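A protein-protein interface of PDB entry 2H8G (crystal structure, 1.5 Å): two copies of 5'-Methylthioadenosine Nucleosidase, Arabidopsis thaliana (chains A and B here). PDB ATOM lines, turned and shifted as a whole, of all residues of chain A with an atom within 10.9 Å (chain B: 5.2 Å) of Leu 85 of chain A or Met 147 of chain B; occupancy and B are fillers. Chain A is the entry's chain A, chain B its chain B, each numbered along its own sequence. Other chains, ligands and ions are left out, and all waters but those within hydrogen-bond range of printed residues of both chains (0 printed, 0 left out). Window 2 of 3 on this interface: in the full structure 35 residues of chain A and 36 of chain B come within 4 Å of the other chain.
No position is printed for both chains.
Of the 10 pairs that touch across the chains among the printed residues, none has its exchanged pair printed and touching as well.
N of Leu 85 of chain A lies within hydrogen-bond range of OD2 of Asp 82 of chain A (2.9 Å).
The side-chain hydroxyl (OG) of Ser 89 of chain A is in hydrogen-bond range of the backbone NH (N) of Asp 82 of chain A (3.5 Å).
The backbone carbonyl oxygen (O) of Gly 80 of chain A sits at hydrogen-bond distance from the backbone NH (N) of Ser 89 of chain A (2.9 Å).
The backbone NH (N) of Asp 82 of chain A sits at hydrogen-bond distance from the backbone carbonyl oxygen (O) of Ile 87 of chain A (2.8 Å).
The backbone NH (N) of Gln 36 of chain A sits at hydrogen-bond distance from the side-chain carboxylate (OD1) of Asp 88 of chain A (3.0 Å).
The backbone NH of Met 147 of chain B sits close to the side-chain carboxylate of Asp 149 of chain B, at 3.5 Å.
Among the printed residues, pairs that only touch across the chains: Asp 82 of chain A with Tyr 151 of chain B (3.7 Å), Leu 85 of chain A with Met 147 of chain B (3.5 Å), Leu 85 of chain A with Leu 150 of chain B (3.97 Å), Ile 87 of chain A with Met 147 of chain B (3.9 Å), Ile 87 of chain A with Phe 148 of chain B (3.5 Å), Ile 87 of chain A with Tyr 151 of chain B (3.7 Å), Asp 88 of chain A with Phe 148 of chain B (3.6 Å), Ser 89 of chain A with Tyr 151 of chain B (3.2 Å) and Leu 181 of chain A with Ile 145 of chain B (3.7 Å).
Of the 7 printed residues of chain B, 5 touch a printed residue of chain A.
Hydrophobic or aromatic side chains of chain B that line the printed part of chain A: Ile 145, Met 147, Phe 148, Leu 150 and Tyr 151.
Of the 17 printed residues of chain A, 7 touch a printed residue of chain B.
Printed residues of chain A that touch a printed residue of chain B: Asp 82, Leu 85, Ile 87, Asp 88, Ser 89, Val 90 and Leu 181.
Hydrophobic or aromatic side chains of chain A that line the printed part of chain B: Leu 85, Ile 87, Val 90 and Leu 181.
Among the printed residues, 10 pairs touch across the chains.
Among the printed residues, no Asp or Glu carboxylate lies within 4 Å of a Lys or Arg side-chain nitrogen of the other chain.
Of the printed residues of chain B, Ser 89 of chain A touches Tyr 151 (3.2 Å).
No residue of chain A comes within 4 Å of Pro 146 of chain B.
Phe 148 of chain B touches just these residues of chain A: Ile 87 and Asp 88.
Printed residues of chain A within 4 Å of Leu 150 of chain B: Leu 85.
Of the printed residues of chain A, Tyr 151 of chain B touches Asp 82 (3.7 Å), Ile 87 (3.7 Å), Ser 89 (3.2 Å) and Val 90 (2.6 Å).
The nearest residue of chain B that does not touch Leu 85 of chain A is Tyr 151 of chain B (4.2 Å).
The nearest printed residue of chain B that does not touch Ser 89 of chain A is Phe 148 of chain B (5.8 Å).
O of Val 90 of chain A lies within hydrogen-bond range of OH of Tyr 151 of chain B (2.6 Å).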
ATOM      1  N   GLN A  36     -35.591   1.736 -12.120  1.00  0.00           N
ATOM      2  CA  GLN A  36     -36.814   0.969 -12.337  1.00  0.00           C
ATOM      3  C   GLN A  36     -36.959  -0.079 -11.237  1.00  0.00           C
ATOM      4  O   GLN A  36     -38.072  -0.393 -10.818  1.00  0.00           O
ATOM      5  CB  GLN A  36     -36.780   0.261 -13.696  1.00  0.00           C
ATOM      6  CG  GLN A  36     -35.927  -1.001 -13.715  1.00  0.00           C
ATOM      7  CD  GLN A  36     -36.343  -1.980 -14.802  1.00  0.00           C
ATOM      8  OE1 GLN A  36     -37.516  -2.337 -14.917  1.00  0.00           O
ATOM      9  NE2 GLN A  36     -35.379  -2.423 -15.602  1.00  0.00           N
ATOM     10  N   PRO A  61     -37.227   8.124 -23.265  1.00  0.00           N
ATOM     11  CA  PRO A  61     -37.120   6.829 -22.588  1.00  0.00           C
ATOM     12  C   PRO A  61     -37.799   6.820 -21.222  1.00  0.00           C
ATOM     13  O   PRO A  61     -37.864   5.783 -20.562  1.00  0.00           O
ATOM     14  CB  PRO A  61     -35.616   6.632 -22.479  1.00  0.00           C
ATOM     15  CG  PRO A  61     -35.142   8.026 -22.231  1.00  0.00           C
ATOM     16  CD  PRO A  61     -35.933   8.831 -23.238  1.00  0.00           C
ATOM     17  N   GLY A  80     -35.825   6.000 -16.880  1.00  0.00           N
ATOM     18  CA  GLY A  80     -35.734   4.901 -17.825  1.00  0.00           C
ATOM     19  C   GLY A  80     -34.340   4.486 -18.246  1.00  0.00           C
ATOM     20  O   GLY A  80     -33.337   4.942 -17.694  1.00  0.00           O
ATOM     21  N   ARG A  81     -34.284   3.616 -19.247  1.00  0.00           N
ATOM     22  CA  ARG A  81     -33.024   3.100 -19.761  1.00  0.00           C
ATOM     23  C   ARG A  81     -32.299   4.084 -20.666  1.00  0.00           C
ATOM     24  O   ARG A  81     -32.907   4.750 -21.506  1.00  0.00           O
ATOM     25  CB  ARG A  81     -33.269   1.813 -20.547  1.00  0.00           C
ATOM     26  CG  ARG A  81     -34.191   0.827 -19.856  1.00  0.00           C
ATOM     27  CD  ARG A  81     -35.114   0.138 -20.854  1.00  0.00           C
ATOM     28  NE  ARG A  81     -35.875   1.104 -21.645  1.00  0.00           N
ATOM     29  CZ  ARG A  81     -35.425   1.700 -22.747  1.00  0.00           C
ATOM     30  NH1 ARG A  81     -34.210   1.427 -23.205  1.00  0.00           N
ATOM     31  NH2 ARG A  81     -36.187   2.579 -23.387  1.00  0.00           N
ATOM     32  N   ASP A  82     -30.989   4.165 -20.484  1.00  0.00           N
ATOM     33  CA  ASP A  82     -30.157   5.029 -21.302  1.00  0.00           C
ATOM     34  C   ASP A  82     -30.051   4.344 -22.661  1.00  0.00           C
ATOM     35  O   ASP A  82     -29.728   3.159 -22.736  1.00  0.00           O
ATOM     36  CB  ASP A  82     -28.768   5.160 -20.684  1.00  0.00           C
ATOM     37  CG  ASP A  82     -27.841   6.004 -21.525  1.00  0.00           C
ATOM     38  OD1 ASP A  82     -28.118   7.209 -21.673  1.00  0.00           O
ATOM     39  OD2 ASP A  82     -26.841   5.462 -22.045  1.00  0.00           O
ATOM     40  N   ALA A  83     -30.324   5.081 -23.731  1.00  0.00           N
ATOM     41  CA  ALA A  83     -30.268   4.510 -25.073  1.00  0.00           C
ATOM     42  C   ALA A  83     -28.913   3.895 -25.423  1.00  0.00           C
ATOM     43  O   ALA A  83     -28.851   2.832 -26.043  1.00  0.00           O
ATOM     44  CB  ALA A  83     -30.639   5.572 -26.107  1.00  0.00           C
ATOM     45  N   ALA A  84     -27.834   4.557 -25.018  1.00  0.00           N
ATOM     46  CA  ALA A  84     -26.486   4.083 -25.323  1.00  0.00           C
ATOM     47  C   ALA A  84     -25.984   2.899 -24.501  1.00  0.00           C
ATOM     48  O   ALA A  84     -25.403   1.966 -25.055  1.00  0.00           O
ATOM     49  CB  ALA A  84     -25.492   5.243 -25.212  1.00  0.00           C
ATOM     50  N   LEU A  85     -26.195   2.929 -23.188  1.00  0.00           N
ATOM     51  CA  LEU A  85     -25.714   1.853 -22.327  1.00  0.00           C
ATOM     52  C   LEU A  85     -26.784   0.903 -21.795  1.00  0.00           C
ATOM     53  O   LEU A  85     -26.461  -0.184 -21.323  1.00  0.00           O
ATOM     54  CB  LEU A  85     -24.919   2.429 -21.149  1.00  0.00           C
ATOM     55  CG  LEU A  85     -23.526   3.020 -21.409  1.00  0.00           C
ATOM     56  CD1 LEU A  85     -22.632   1.959 -22.040  1.00  0.00           C
ATOM     57  CD2 LEU A  85     -23.628   4.233 -22.311  1.00  0.00           C
ATOM     58  N   GLY A  86     -28.048   1.318 -21.854  1.00  0.00           N
ATOM     59  CA  GLY A  86     -29.133   0.470 -21.385  1.00  0.00           C
ATOM     60  C   GLY A  86     -29.517   0.563 -19.913  1.00  0.00           C
ATOM     61  O   GLY A  86     -30.667   0.298 -19.555  1.00  0.00           O
ATOM     62  N   ILE A  87     -28.570   0.932 -19.057  1.00  0.00           N
ATOM     63  CA  ILE A  87     -28.833   1.035 -17.625  1.00  0.00           C
ATOM     64  C   ILE A  87     -29.718   2.228 -17.252  1.00  0.00           C
ATOM     65  O   ILE A  87     -30.000   3.090 -18.087  1.00  0.00           O
ATOM     66  CB  ILE A  87     -27.499   1.096 -16.830  1.00  0.00           C
ATOM     67  CG1 ILE A  87     -26.559   2.150 -17.429  1.00  0.00           C
ATOM     68  CG2 ILE A  87     -26.806  -0.261 -16.877  1.00  0.00           C
ATOM     69  CD1 ILE A  87     -27.000   3.580 -17.232  1.00  0.00           C
ATOM     70  N   ASP A  88     -30.161   2.264 -15.996  1.00  0.00           N
ATOM     71  CA  ASP A  88     -31.005   3.355 -15.514  1.00  0.00           C
ATOM     72  C   ASP A  88     -30.271   4.676 -15.652  1.00  0.00           C
ATOM     73  O   ASP A  88     -29.086   4.773 -15.327  1.00  0.00           O
ATOM     74  CB  ASP A  88     -31.363   3.163 -14.040  1.00  0.00           C
ATOM     75  CG  ASP A  88     -32.374   2.064 -13.818  1.00  0.00           C
ATOM     76  OD1 ASP A  88     -33.525   2.200 -14.285  1.00  0.00           O
ATOM     77  OD2 ASP A  88     -32.012   1.066 -13.163  1.00  0.00           O
ATOM     78  N   SER A  89     -30.988   5.691 -16.115  1.00  0.00           N
ATOM     79  CA  SER A  89     -30.412   7.016 -16.303  1.00  0.00           C
ATOM     80  C   SER A  89     -30.413   7.775 -14.983  1.00  0.00           C
ATOM     81  O   SER A  89     -31.222   8.680 -14.772  1.00  0.00           O
ATOM     82  CB  SER A  89     -31.213   7.784 -17.353  1.00  0.00           C
ATOM     83  OG  SER A  89     -31.188   7.102 -18.599  1.00  0.00           O
ATOM     84  N   VAL A  90     -29.493   7.391 -14.106  1.00  0.00           N
ATOM     85  CA  VAL A  90     -29.359   7.997 -12.790  1.00  0.00           C
ATOM     86  C   VAL A  90     -28.642   9.347 -12.856  1.00  0.00           C
ATOM     87  O   VAL A  90     -28.149   9.752 -13.905  1.00  0.00           O
ATOM     88  CB  VAL A  90     -28.574   7.062 -11.828  1.00  0.00           C
ATOM     89  CG1 VAL A  90     -29.318   5.741 -11.659  1.00  0.00           C
ATOM     90  CG2 VAL A  90     -27.173   6.802 -12.367  1.00  0.00           C
ATOM     91  N   LEU A 181     -21.082   7.990  -7.361  1.00  0.00           N
ATOM     92  CA  LEU A 181     -21.500   6.958  -6.425  1.00  0.00           C
ATOM     93  C   LEU A 181     -20.410   6.756  -5.385  1.00  0.00           C
ATOM     94  O   LEU A 181     -20.689   6.400  -4.243  1.00  0.00           O
ATOM     95  CB  LEU A 181     -21.765   5.653  -7.177  1.00  0.00           C
ATOM     96  CG  LEU A 181     -22.104   4.443  -6.304  1.00  0.00           C
ATOM     97  CD1 LEU A 181     -23.373   4.702  -5.517  1.00  0.00           C
ATOM     98  CD2 LEU A 181     -22.264   3.214  -7.182  1.00  0.00           C
ATOM     99  N   MET A 201     -27.710  10.517  -5.267  1.00  0.00           N
ATOM    100  CA  MET A 201     -27.334  11.112  -6.537  1.00  0.00           C
ATOM    101  C   MET A 201     -28.409  11.936  -7.240  1.00  0.00           C
ATOM    102  O   MET A 201     -28.180  12.392  -8.358  1.00  0.00           O
ATOM    103  CB  MET A 201     -26.831  10.009  -7.481  1.00  0.00           C
ATOM    104  CG  MET A 201     -25.562   9.325  -6.994  1.00  0.00           C
ATOM    105  SD  MET A 201     -25.141   7.817  -7.892  1.00  0.00           S
ATOM    106  CE  MET A 201     -24.748   8.479  -9.475  1.00  0.00           C
ATOM    107  N   ALA A 234     -19.942   0.300  -3.869  1.00  0.00           N
ATOM    108  CA  ALA A 234     -20.682  -0.318  -4.961  1.00  0.00           C
ATOM    109  C   ALA A 234     -21.114  -1.735  -4.593  1.00  0.00           C
ATOM    110  O   ALA A 234     -22.259  -2.127  -4.832  1.00  0.00           O
ATOM    111  CB  ALA A 234     -19.829  -0.334  -6.226  1.00  0.00           C
ATOM    112  N   LEU A 238     -25.156  -2.694  -4.154  1.00  0.00           N
ATOM    113  CA  LEU A 238     -25.825  -3.676  -4.998  1.00  0.00           C
ATOM    114  C   LEU A 238     -26.234  -4.934  -4.237  1.00  0.00           C
ATOM    115  O   LEU A 238     -27.251  -5.552  -4.546  1.00  0.00           O
ATOM    116  CB  LEU A 238     -24.922  -4.043  -6.178  1.00  0.00           C
ATOM    117  CG  LEU A 238     -24.516  -2.847  -7.050  1.00  0.00           C
ATOM    118  CD1 LEU A 238     -23.477  -3.282  -8.075  1.00  0.00           C
ATOM    119  CD2 LEU A 238     -25.748  -2.261  -7.732  1.00  0.00           C
ATOM    120  N   ILE B 145     -19.372   1.134 -11.752  1.00  0.00           N
ATOM    121  CA  ILE B 145     -20.176  -0.031 -12.111  1.00  0.00           C
ATOM    122  C   ILE B 145     -20.076  -0.125 -13.638  1.00  0.00           C
ATOM    123  O   ILE B 145     -20.372   0.835 -14.345  1.00  0.00           O
ATOM    124  CB  ILE B 145     -21.649   0.143 -11.664  1.00  0.00           C
ATOM    125  CG1 ILE B 145     -21.710   0.288 -10.138  1.00  0.00           C
ATOM    126  CG2 ILE B 145     -22.481  -1.069 -12.093  1.00  0.00           C
ATOM    127  CD1 ILE B 145     -23.103   0.570  -9.598  1.00  0.00           C
ATOM    128  N   PRO B 146     -19.652  -1.292 -14.159  1.00  0.00           N
ATOM    129  CA  PRO B 146     -19.453  -1.642 -15.571  1.00  0.00           C
ATOM    130  C   PRO B 146     -19.961  -0.763 -16.719  1.00  0.00           C
ATOM    131  O   PRO B 146     -19.173  -0.328 -17.557  1.00  0.00           O
ATOM    132  CB  PRO B 146     -20.000  -3.058 -15.631  1.00  0.00           C
ATOM    133  CG  PRO B 146     -19.417  -3.626 -14.379  1.00  0.00           C
ATOM    134  CD  PRO B 146     -19.671  -2.522 -13.342  1.00  0.00           C
ATOM    135  N   MET B 147     -21.265  -0.528 -16.777  1.00  0.00           N
ATOM    136  CA  MET B 147     -21.867   0.276 -17.837  1.00  0.00           C
ATOM    137  C   MET B 147     -22.196   1.684 -17.348  1.00  0.00           C
ATOM    138  O   MET B 147     -22.203   2.646 -18.125  1.00  0.00           O
ATOM    139  CB  MET B 147     -23.140  -0.410 -18.337  1.00  0.00           C
ATOM    140  CG  MET B 147     -22.920  -1.838 -18.828  1.00  0.00           C
ATOM    141  SD  MET B 147     -21.805  -1.900 -20.238  1.00  0.00           S
ATOM    142  CE  MET B 147     -22.923  -1.449 -21.536  1.00  0.00           C
ATOM    143  N   PHE B 148     -22.487   1.798 -16.057  1.00  0.00           N
ATOM    144  CA  PHE B 148     -22.798   3.094 -15.468  1.00  0.00           C
ATOM    145  C   PHE B 148     -21.597   4.019 -15.578  1.00  0.00           C
ATOM    146  O   PHE B 148     -21.749   5.242 -15.660  1.00  0.00           O
ATOM    147  CB  PHE B 148     -23.171   2.943 -13.996  1.00  0.00           C
ATOM    148  CG  PHE B 148     -24.546   2.395 -13.769  1.00  0.00           C
ATOM    149  CD1 PHE B 148     -24.777   1.023 -13.772  1.00  0.00           C
ATOM    150  CD2 PHE B 148     -25.614   3.256 -13.546  1.00  0.00           C
ATOM    151  CE1 PHE B 148     -26.057   0.518 -13.552  1.00  0.00           C
ATOM    152  CE2 PHE B 148     -26.896   2.762 -13.326  1.00  0.00           C
ATOM    153  CZ  PHE B 148     -27.117   1.389 -13.329  1.00  0.00           C
ATOM    154  N   ASP B 149     -20.403   3.438 -15.568  1.00  0.00           N
ATOM    155  CA  ASP B 149     -19.193   4.238 -15.667  1.00  0.00           C
ATOM    156  C   ASP B 149     -19.161   5.027 -16.974  1.00  0.00           C
ATOM    157  O   ASP B 149     -18.976   6.244 -16.962  1.00  0.00           O
ATOM    158  CB  ASP B 149     -17.940   3.357 -15.517  1.00  0.00           C
ATOM    159  CG  ASP B 149     -17.975   2.105 -16.382  1.00  0.00           C
ATOM    160  OD1 ASP B 149     -17.075   1.255 -16.210  1.00  0.00           O
ATOM    161  OD2 ASP B 149     -18.882   1.963 -17.225  1.00  0.00           O
ATOM    162  N   LEU B 150     -19.361   4.341 -18.095  1.00  0.00           N
ATOM    163  CA  LEU B 150     -19.376   4.997 -19.400  1.00  0.00           C
ATOM    164  C   LEU B 150     -20.546   5.980 -19.479  1.00  0.00           C
ATOM    165  O   LEU B 150     -20.480   6.993 -20.177  1.00  0.00           O
ATOM    166  CB  LEU B 150     -19.502   3.948 -20.508  1.00  0.00           C
ATOM    167  CG  LEU B 150     -18.326   2.971 -20.619  1.00  0.00           C
ATOM    168  CD1 LEU B 150     -18.693   1.817 -21.540  1.00  0.00           C
ATOM    169  CD2 LEU B 150     -17.102   3.707 -21.140  1.00  0.00           C
ATOM    170  N   TYR B 151     -21.620   5.670 -18.764  1.00  0.00           N
ATOM    171  CA  TYR B 151     -22.798   6.528 -18.746  1.00  0.00           C
ATOM    172  C   TYR B 151     -22.463   7.847 -18.050  1.00  0.00           C
ATOM    173  O   TYR B 151     -22.826   8.924 -18.528  1.00  0.00           O
ATOM    174  CB  TYR B 151     -23.940   5.826 -18.010  1.00  0.00           C
ATOM    175  CG  TYR B 151     -25.066   6.746 -17.605  1.00  0.00           C
ATOM    176  CD1 TYR B 151     -26.016   7.177 -18.530  1.00  0.00           C
ATOM    177  CD2 TYR B 151     -25.165   7.204 -16.293  1.00  0.00           C
ATOM    178  CE1 TYR B 151     -27.042   8.047 -18.157  1.00  0.00           C
ATOM    179  CE2 TYR B 151     -26.180   8.071 -15.910  1.00  0.00           C
ATOM    180  CZ  TYR B 151     -27.112   8.487 -16.843  1.00  0.00           C
ATOM    181  OH  TYR B 151     -28.111   9.353 -16.459  1.00  0.00           O
